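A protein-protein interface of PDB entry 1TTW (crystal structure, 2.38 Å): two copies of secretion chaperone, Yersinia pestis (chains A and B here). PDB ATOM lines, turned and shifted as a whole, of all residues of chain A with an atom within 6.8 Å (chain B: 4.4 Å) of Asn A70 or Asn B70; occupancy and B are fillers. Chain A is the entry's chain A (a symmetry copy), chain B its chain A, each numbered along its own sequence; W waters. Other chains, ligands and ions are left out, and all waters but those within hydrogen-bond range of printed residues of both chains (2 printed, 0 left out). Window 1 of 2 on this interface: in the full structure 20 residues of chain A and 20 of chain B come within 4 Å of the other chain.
Leu A67 touches Cys B81, and with the chains exchanged Cys A81 touches Leu B67.
Asn B70 touches its own counterpart, Asn A70.
Asn A70 touches Trp B92, and with the chains exchanged Trp A92 touches Asn B70.
Arg A80 touches Trp B92, and with the chains exchanged Trp A92 touches Arg B80.
10 positions are printed for both chains.
Of the 19 pairs that touch across the chains among the printed residues, 16 have their exchanged pair printed and touching as well.
O of Ala A82 is in hydrogen-bond range of N of Leu A90 (2.7 Å).
The backbone carbonyl oxygen of Trp A92 lies within hydrogen-bond range of the backbone NH of Arg A80, 2.8 Å away.
N of Arg B80 is in hydrogen-bond range of O of Trp B92 (2.8 Å).
NH2 of Arg B80 is in hydrogen-bond range of O of Leu B71, 2.6 Å away.
O of Leu A71 lies within hydrogen-bond range of NH2 of Arg A80, at 2.6 Å.
CD2 of Leu B67 touches CD2 of Leu A67, at 3.0 Å.
Leu A67 touches Ala B82 (O to CA, 2.9 Å).
Asn A70 touches Ala B82.
Phe A72 touches Trp B92 (CB to CE3, 3.4 Å).
Trp B92 touches Arg A80.
Cys A81 touches Leu B67 (O to CD1, 3.6 Å).
Ala A82 touches Leu B67.
Ala A82 touches Asn B70.
CA of Arg B68 touches O of Leu A83 (3.5 Å).
Arg B80 touches Trp A92 (NH2 to CH2, 3.4 Å).
Asn B70 touches just these residues of chain A: Asn A70, Cys A81, Ala A82 and Trp A92.
Of the printed residues of chain A, Trp B92 touches Asn A70 (2.8 Å), Leu A71 (3.5 Å), Phe A72 (3.4 Å) and Arg A80 (3.4 Å).
Printed residues of chain B within 4 Å of Ala A82: Leu B67 and Asn B70.
The nearest residue of chain B that does not touch Asn A70 is Arg B80 (4.2 Å).
Water W2 lies within hydrogen-bond range of OD1 of Asn B70 (2.7 Å), N of Cys B81 (2.7 Å) and ND2 of Asn A70 (3.2 Å).
Water W1 lies within hydrogen-bond range of the side-chain amide oxygen of Asn A70 (2.7 Å), the backbone NH of Cys A81 (2.7 Å) and the side-chain amide nitrogen of Asn B70 (3.2 Å).
Hydrophobic or aromatic side chains of chain B that line the printed part of chain A: Leu B67, Ala B82 and Trp B92.
Hydrophobic or aromatic side chains of chain A within 4 Å of the printed part of chain B: Leu A67, Phe A72, Ala A82, Leu A83 and Trp A92.
Among the printed residues, no Asp or Glu carboxylate lies within 4 Å of a Lys or Arg side-chain nitrogen of the other chain.
The indole nitrogen (NE1) of Trp A92 is in hydrogen-bond range of the backbone carbonyl oxygen (O) of Asn B70 (2.8 Å).
The side-chain amide nitrogen of Asn B70 sits at hydrogen-bond distance from the side-chain amide oxygen of Asn A70 (3.2 Å).
The backbone carbonyl oxygen (O) of Leu B67 sits at hydrogen-bond distance from the backbone NH (N) of Leu A83 (3.0 Å).
NE1 of Trp B92 lies within hydrogen-bond range of O of Asn A70, at 2.8 Å.
O of Cys B81 sits at hydrogen-bond distance from ND2 of Asn A70 (2.6 Å).
The side-chain amide nitrogen of Asn B70 is in hydrogen-bond range of the backbone carbonyl oxygen of Cys A81 (2.6 Å).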
ATOM      1  N   ASP A  65      11.380  23.142   5.241  1.00  0.00           N
ATOM      2  CA  ASP A  65      10.393  24.129   4.719  1.00  0.00           C
ATOM      3  C   ASP A  65       8.941  23.662   4.923  1.00  0.00           C
ATOM      4  O   ASP A  65       8.066  24.407   5.228  1.00  0.00           O
ATOM      5  CB  ASP A  65      10.694  24.477   3.230  1.00  0.00           C
ATOM      6  CG  ASP A  65      12.190  24.920   3.037  1.00  0.00           C
ATOM      7  OD1 ASP A  65      13.043  24.099   2.508  1.00  0.00           O
ATOM      8  OD2 ASP A  65      12.597  26.024   3.505  1.00  0.00           O
ATOM      9  N   ILE A  66       8.689  22.408   4.678  1.00  0.00           N
ATOM     10  CA  ILE A  66       7.431  21.813   5.076  1.00  0.00           C
ATOM     11  C   ILE A  66       7.218  21.909   6.605  1.00  0.00           C
ATOM     12  O   ILE A  66       6.283  22.598   7.012  1.00  0.00           O
ATOM     13  CB  ILE A  66       7.425  20.448   4.487  1.00  0.00           C
ATOM     14  CG1 ILE A  66       7.191  20.665   2.970  1.00  0.00           C
ATOM     15  CG2 ILE A  66       6.358  19.696   5.100  1.00  0.00           C
ATOM     16  CD1 ILE A  66       7.604  19.549   2.160  1.00  0.00           C
ATOM     17  N   LEU A  67       8.175  21.424   7.416  1.00  0.00           N
ATOM     18  CA  LEU A  67       8.084  21.525   8.901  1.00  0.00           C
ATOM     19  C   LEU A  67       7.784  22.871   9.461  1.00  0.00           C
ATOM     20  O   LEU A  67       6.982  22.996  10.365  1.00  0.00           O
ATOM     21  CB  LEU A  67       9.345  20.978   9.566  1.00  0.00           C
ATOM     22  CG  LEU A  67       9.072  19.537   9.991  1.00  0.00           C
ATOM     23  CD1 LEU A  67       7.666  18.979   9.864  1.00  0.00           C
ATOM     24  CD2 LEU A  67       9.977  18.687   9.287  1.00  0.00           C
ATOM     25  N   ARG A  68       8.369  23.903   8.878  1.00  0.00           N
ATOM     26  CA  ARG A  68       8.105  25.345   9.186  1.00  0.00           C
ATOM     27  C   ARG A  68       6.678  25.746   8.818  1.00  0.00           C
ATOM     28  O   ARG A  68       6.049  26.546   9.464  1.00  0.00           O
ATOM     29  CB  ARG A  68       9.076  26.188   8.396  1.00  0.00           C
ATOM     30  CG  ARG A  68      10.542  26.018   8.785  1.00  0.00           C
ATOM     31  CD  ARG A  68      11.407  27.378   8.819  1.00  0.00           C
ATOM     32  NE  ARG A  68      12.823  27.174   9.277  1.00  0.00           N
ATOM     33  CZ  ARG A  68      13.848  26.568   8.572  1.00  0.00           C
ATOM     34  NH1 ARG A  68      13.699  26.064   7.348  1.00  0.00           N
ATOM     35  NH2 ARG A  68      15.053  26.461   9.128  1.00  0.00           N
ATOM     36  N   LYS A  69       6.089  25.058   7.855  1.00  0.00           N
ATOM     37  CA  LYS A  69       4.649  25.318   7.503  1.00  0.00           C
ATOM     38  C   LYS A  69       3.581  24.330   8.037  1.00  0.00           C
ATOM     39  O   LYS A  69       2.343  24.385   7.588  1.00  0.00           O
ATOM     40  CB  LYS A  69       4.542  25.372   5.938  1.00  0.00           C
ATOM     41  CG  LYS A  69       5.421  26.544   5.310  1.00  0.00           C
ATOM     42  CD  LYS A  69       5.444  26.489   3.671  1.00  0.00           C
ATOM     43  CE  LYS A  69       6.868  26.223   2.939  1.00  0.00           C
ATOM     44  NZ  LYS A  69       7.256  27.239   1.820  1.00  0.00           N
ATOM     45  N   ASN A  70       4.029  23.402   8.907  1.00  0.00           N
ATOM     46  CA  ASN A  70       3.158  22.327   9.418  1.00  0.00           C
ATOM     47  C   ASN A  70       2.497  22.765  10.708  1.00  0.00           C
ATOM     48  O   ASN A  70       2.564  22.052  11.651  1.00  0.00           O
ATOM     49  CB  ASN A  70       3.976  21.069   9.603  1.00  0.00           C
ATOM     50  CG  ASN A  70       3.171  19.843   9.810  1.00  0.00           C
ATOM     51  OD1 ASN A  70       2.312  19.542   8.942  1.00  0.00           O
ATOM     52  ND2 ASN A  70       3.538  18.971  10.911  1.00  0.00           N
ATOM     53  N   LEU A  71       1.806  23.911  10.682  1.00  0.00           N
ATOM     54  CA  LEU A  71       1.180  24.533  11.773  1.00  0.00           C
ATOM     55  C   LEU A  71      -0.254  24.306  11.654  1.00  0.00           C
ATOM     56  O   LEU A  71      -0.703  23.683  10.660  1.00  0.00           O
ATOM     57  CB  LEU A  71       1.437  25.981  11.760  1.00  0.00           C
ATOM     58  CG  LEU A  71       2.155  26.669  12.920  1.00  0.00           C
ATOM     59  CD1 LEU A  71       1.787  28.257  13.133  1.00  0.00           C
ATOM     60  CD2 LEU A  71       1.878  25.910  14.236  1.00  0.00           C
ATOM     61  N   PHE A  72      -0.977  24.628  12.714  1.00  0.00           N
ATOM     62  CA  PHE A  72      -2.394  24.416  12.691  1.00  0.00           C
ATOM     63  C   PHE A  72      -3.161  25.565  11.940  1.00  0.00           C
ATOM     64  O   PHE A  72      -2.758  26.664  12.010  1.00  0.00           O
ATOM     65  CB  PHE A  72      -2.906  24.454  14.152  1.00  0.00           C
ATOM     66  CG  PHE A  72      -2.234  25.470  14.979  1.00  0.00           C
ATOM     67  CD1 PHE A  72      -2.676  26.830  14.948  1.00  0.00           C
ATOM     68  CD2 PHE A  72      -1.199  25.170  15.784  1.00  0.00           C
ATOM     69  CE1 PHE A  72      -2.157  27.794  15.762  1.00  0.00           C
ATOM     70  CE2 PHE A  72      -0.580  26.191  16.665  1.00  0.00           C
ATOM     71  CZ  PHE A  72      -1.075  27.484  16.629  1.00  0.00           C
ATOM     72  N   ILE A  79      -3.216  21.270   3.238  1.00  0.00           N
ATOM     73  CA  ILE A  79      -2.477  20.196   2.648  1.00  0.00           C
ATOM     74  C   ILE A  79      -1.348  19.876   3.511  1.00  0.00           C
ATOM     75  O   ILE A  79      -0.619  20.758   3.952  1.00  0.00           O
ATOM     76  CB  ILE A  79      -1.843  20.508   1.299  1.00  0.00           C
ATOM     77  CG1 ILE A  79      -2.842  20.972   0.221  1.00  0.00           C
ATOM     78  CG2 ILE A  79      -1.229  19.274   0.696  1.00  0.00           C
ATOM     79  CD1 ILE A  79      -4.081  20.022  -0.083  1.00  0.00           C
ATOM     80  N   ARG A  80      -1.127  18.565   3.756  1.00  0.00           N
ATOM     81  CA  ARG A  80      -0.034  18.197   4.761  1.00  0.00           C
ATOM     82  C   ARG A  80       0.855  17.323   4.046  1.00  0.00           C
ATOM     83  O   ARG A  80       0.355  16.697   3.130  1.00  0.00           O
ATOM     84  CB  ARG A  80      -0.612  17.499   5.990  1.00  0.00           C
ATOM     85  CG  ARG A  80      -1.655  18.328   6.644  1.00  0.00           C
ATOM     86  CD  ARG A  80      -1.041  19.501   7.349  1.00  0.00           C
ATOM     87  NE  ARG A  80      -1.958  20.248   8.313  1.00  0.00           N
ATOM     88  CZ  ARG A  80      -1.605  21.367   8.868  1.00  0.00           C
ATOM     89  NH1 ARG A  80      -0.382  21.811   8.645  1.00  0.00           N
ATOM     90  NH2 ARG A  80      -2.418  21.995   9.719  1.00  0.00           N
ATOM     91  N   CYS A  81       2.140  17.280   4.404  1.00  0.00           N
ATOM     92  CA  CYS A  81       3.091  16.402   3.669  1.00  0.00           C
ATOM     93  C   CYS A  81       3.766  15.479   4.649  1.00  0.00           C
ATOM     94  O   CYS A  81       4.080  15.921   5.741  1.00  0.00           O
ATOM     95  CB  CYS A  81       4.141  17.239   2.957  1.00  0.00           C
ATOM     96  SG  CYS A  81       3.309  18.770   2.229  1.00  0.00           S
ATOM     97  N   ALA A  82       3.932  14.214   4.235  1.00  0.00           N
ATOM     98  CA  ALA A  82       4.689  13.158   4.903  1.00  0.00           C
ATOM     99  C   ALA A  82       5.695  12.636   3.892  1.00  0.00           C
ATOM    100  O   ALA A  82       5.487  12.807   2.622  1.00  0.00           O
ATOM    101  CB  ALA A  82       3.811  11.965   5.236  1.00  0.00           C
ATOM    102  N   LEU A  83       6.671  11.885   4.417  1.00  0.00           N
ATOM    103  CA  LEU A  83       7.379  10.905   3.614  1.00  0.00           C
ATOM    104  C   LEU A  83       6.980   9.438   3.760  1.00  0.00           C
ATOM    105  O   LEU A  83       6.647   8.957   4.832  1.00  0.00           O
ATOM    106  CB  LEU A  83       8.842  11.010   3.896  1.00  0.00           C
ATOM    107  CG  LEU A  83       9.330  12.396   3.653  1.00  0.00           C
ATOM    108  CD1 LEU A  83      10.550  12.613   4.444  1.00  0.00           C
ATOM    109  CD2 LEU A  83       9.546  12.478   2.169  1.00  0.00           C
ATOM    110  N   LEU A  90       4.283  12.237   0.298  1.00  0.00           N
ATOM    111  CA  LEU A  90       2.847  11.892   0.315  1.00  0.00           C
ATOM    112  C   LEU A  90       2.102  13.101   0.862  1.00  0.00           C
ATOM    113  O   LEU A  90       2.386  13.608   1.907  1.00  0.00           O
ATOM    114  CB  LEU A  90       2.587  10.756   1.260  1.00  0.00           C
ATOM    115  CG  LEU A  90       1.529   9.766   0.909  1.00  0.00           C
ATOM    116  CD1 LEU A  90       1.937   8.530   1.697  1.00  0.00           C
ATOM    117  CD2 LEU A  90       0.122  10.291   1.288  1.00  0.00           C
ATOM    118  N   TRP A  92      -1.726  15.097   1.791  1.00  0.00           N
ATOM    119  CA  TRP A  92      -3.064  14.614   2.059  1.00  0.00           C
ATOM    120  C   TRP A  92      -3.761  15.727   2.722  1.00  0.00           C
ATOM    121  O   TRP A  92      -3.167  16.691   3.158  1.00  0.00           O
ATOM    122  CB  TRP A  92      -2.864  13.343   3.068  1.00  0.00           C
ATOM    123  CG  TRP A  92      -2.098  13.695   4.363  1.00  0.00           C
ATOM    124  CD1 TRP A  92      -0.738  13.594   4.562  1.00  0.00           C
ATOM    125  CD2 TRP A  92      -2.628  14.262   5.593  1.00  0.00           C
ATOM    126  NE1 TRP A  92      -0.412  13.946   5.850  1.00  0.00           N
ATOM    127  CE2 TRP A  92      -1.571  14.309   6.522  1.00  0.00           C
ATOM    128  CE3 TRP A  92      -3.913  14.499   6.064  1.00  0.00           C
ATOM    129  CZ2 TRP A  92      -1.721  14.836   7.806  1.00  0.00           C
ATOM    130  CZ3 TRP A  92      -4.088  15.034   7.344  1.00  0.00           C
ATOM    131  CH2 TRP A  92      -3.035  15.139   8.260  1.00  0.00           C
ATOM    132  N   ILE B  66       9.844  12.834  12.008  1.00  0.00           N
ATOM    133  CA  ILE B  66       8.555  13.489  12.088  1.00  0.00           C
ATOM    134  C   ILE B  66       7.797  13.415  10.741  1.00  0.00           C
ATOM    135  O   ILE B  66       6.749  12.773  10.707  1.00  0.00           O
ATOM    136  CB  ILE B  66       8.824  14.848  12.628  1.00  0.00           C
ATOM    137  CG1 ILE B  66       9.147  14.628  14.129  1.00  0.00           C
ATOM    138  CG2 ILE B  66       7.643  15.652  12.437  1.00  0.00           C
ATOM    139  CD1 ILE B  66       9.876  15.718  14.724  1.00  0.00           C
ATOM    140  N   LEU B  67       8.416  13.863   9.635  1.00  0.00           N
ATOM    141  CA  LEU B  67       7.788  13.779   8.285  1.00  0.00           C
ATOM    142  C   LEU B  67       7.246  12.453   7.883  1.00  0.00           C
ATOM    143  O   LEU B  67       6.165  12.372   7.333  1.00  0.00           O
ATOM    144  CB  LEU B  67       8.745  14.275   7.202  1.00  0.00           C
ATOM    145  CG  LEU B  67       8.401  15.730   6.893  1.00  0.00           C
ATOM    146  CD1 LEU B  67       7.164  16.349   7.518  1.00  0.00           C
ATOM    147  CD2 LEU B  67       9.537  16.532   7.215  1.00  0.00           C
ATOM    148  N   ARG B  68       7.955  11.391   8.223  1.00  0.00           N
ATOM    149  CA  ARG B  68       7.532   9.964   8.043  1.00  0.00           C
ATOM    150  C   ARG B  68       6.320   9.625   8.908  1.00  0.00           C
ATOM    151  O   ARG B  68       5.463   8.860   8.541  1.00  0.00           O
ATOM    152  CB  ARG B  68       8.685   9.072   8.435  1.00  0.00           C
ATOM    153  CG  ARG B  68       9.916   9.180   7.539  1.00  0.00           C
ATOM    154  CD  ARG B  68      10.648   7.783   7.205  1.00  0.00           C
ATOM    155  NE  ARG B  68      11.809   7.927   6.263  1.00  0.00           N
ATOM    156  CZ  ARG B  68      13.046   8.481   6.542  1.00  0.00           C
ATOM    157  NH1 ARG B  68      13.375   8.980   7.733  1.00  0.00           N
ATOM    158  NH2 ARG B  68      13.971   8.539   5.586  1.00  0.00           N
ATOM    159  N   LYS B  69       6.152  10.331  10.013  1.00  0.00           N
ATOM    160  CA  LYS B  69       4.927  10.133  10.866  1.00  0.00           C
ATOM    161  C   LYS B  69       3.784  11.172  10.747  1.00  0.00           C
ATOM    162  O   LYS B  69       2.793  11.170  11.615  1.00  0.00           O
ATOM    163  CB  LYS B  69       5.394  10.070  12.363  1.00  0.00           C
ATOM    164  CG  LYS B  69       6.387   8.855  12.639  1.00  0.00           C
ATOM    165  CD  LYS B  69       7.006   8.895  14.158  1.00  0.00           C
ATOM    166  CE  LYS B  69       8.608   9.091  14.321  1.00  0.00           C
ATOM    167  NZ  LYS B  69       9.330   8.049  15.232  1.00  0.00           N
ATOM    168  N   ASN B  70       3.927  12.087   9.766  1.00  0.00           N
ATOM    169  CA  ASN B  70       2.979  13.204   9.597  1.00  0.00           C
ATOM    170  C   ASN B  70       1.877  12.807   8.638  1.00  0.00           C
ATOM    171  O   ASN B  70       1.629  13.524   7.730  1.00  0.00           O
ATOM    172  CB  ASN B  70       3.730  14.426   9.117  1.00  0.00           C
ATOM    173  CG  ASN B  70       2.961  15.688   9.206  1.00  0.00           C
ATOM    174  OD1 ASN B  70       2.490  16.020  10.324  1.00  0.00           O
ATOM    175  ND2 ASN B  70       2.942  16.552   8.039  1.00  0.00           N
ATOM    176  N   LEU B  71       1.191  11.693   8.924  1.00  0.00           N
ATOM    177  CA  LEU B  71       0.185  11.109   8.138  1.00  0.00           C
ATOM    178  C   LEU B  71      -1.096  11.399   8.768  1.00  0.00           C
ATOM    179  O   LEU B  71      -1.125  12.033   9.852  1.00  0.00           O
ATOM    180  CB  LEU B  71       0.364   9.650   8.070  1.00  0.00           C
ATOM    181  CG  LEU B  71       0.580   8.941   6.734  1.00  0.00           C
ATOM    182  CD1 LEU B  71       0.090   7.373   6.683  1.00  0.00           C
ATOM    183  CD2 LEU B  71      -0.120   9.722   5.602  1.00  0.00           C
ATOM    184  N   ARG B  80       1.214  17.107  16.395  1.00  0.00           N
ATOM    185  CA  ARG B  80       1.883  17.434  15.059  1.00  0.00           C
ATOM    186  C   ARG B  80       3.010  18.260  15.396  1.00  0.00           C
ATOM    187  O   ARG B  80       2.904  18.900  16.426  1.00  0.00           O
ATOM    188  CB  ARG B  80       0.930  18.168  14.118  1.00  0.00           C
ATOM    189  CG  ARG B  80      -0.315  17.392  13.895  1.00  0.00           C
ATOM    190  CD  ARG B  80      -0.051  16.198  13.024  1.00  0.00           C
ATOM    191  NE  ARG B  80      -1.288  15.501  12.466  1.00  0.00           N
ATOM    192  CZ  ARG B  80      -1.211  14.372  11.829  1.00  0.00           C
ATOM    193  NH1 ARG B  80      -0.012  13.871  11.597  1.00  0.00           N
ATOM    194  NH2 ARG B  80      -2.305  13.788  11.337  1.00  0.00           N
ATOM    195  N   CYS B  81       4.078  18.248  14.596  1.00  0.00           N
ATOM    196  CA  CYS B  81       5.269  19.077  14.929  1.00  0.00           C
ATOM    197  C   CYS B  81       5.583  19.978  13.762  1.00  0.00           C
ATOM    198  O   CYS B  81       5.459  19.531  12.635  1.00  0.00           O
ATOM    199  CB  CYS B  81       6.467  18.188  15.218  1.00  0.00           C
ATOM    200  SG  CYS B  81       5.889  16.690  16.211  1.00  0.00           S
ATOM    201  N   ALA B  82       5.945  21.230  14.077  1.00  0.00           N
ATOM    202  CA  ALA B  82       6.454  22.257  13.171  1.00  0.00           C
ATOM    203  C   ALA B  82       7.781  22.724  13.744  1.00  0.00           C
ATOM    204  O   ALA B  82       8.040  22.552  15.005  1.00  0.00           O
ATOM    205  CB  ALA B  82       5.571  23.490  13.170  1.00  0.00           C
ATOM    206  N   TRP B  92       1.525  20.581  18.416  1.00  0.00           N
ATOM    207  CA  TRP B  92       0.204  21.126  18.647  1.00  0.00           C
ATOM    208  C   TRP B  92      -0.735  20.051  18.291  1.00  0.00           C
ATOM    209  O   TRP B  92      -0.383  19.065  17.678  1.00  0.00           O
ATOM    210  CB  TRP B  92       0.081  22.395  17.623  1.00  0.00           C
ATOM    211  CG  TRP B  92       0.309  22.020  16.142  1.00  0.00           C
ATOM    212  CD1 TRP B  92       1.507  22.062  15.462  1.00  0.00           C
ATOM    213  CD2 TRP B  92      -0.656  21.487  15.192  1.00  0.00           C
ATOM    214  NE1 TRP B  92       1.327  21.707  14.146  1.00  0.00           N
ATOM    215  CE2 TRP B  92      -0.012  21.401  13.944  1.00  0.00           C
ATOM    216  CE3 TRP B  92      -2.034  21.313  15.222  1.00  0.00           C
ATOM    217  CZ2 TRP B  92      -0.640  20.892  12.807  1.00  0.00           C
ATOM    218  CZ3 TRP B  92      -2.685  20.796  14.097  1.00  0.00           C
ATOM    219  CH2 TRP B  92      -2.042  20.653  12.863  1.00  0.00           C
HETATM  220  O   HOH W   1       2.519  19.223   6.288  1.00  0.00           O
HETATM  221  O   HOH W   2       3.660  16.307  12.719  1.00  0.00           O
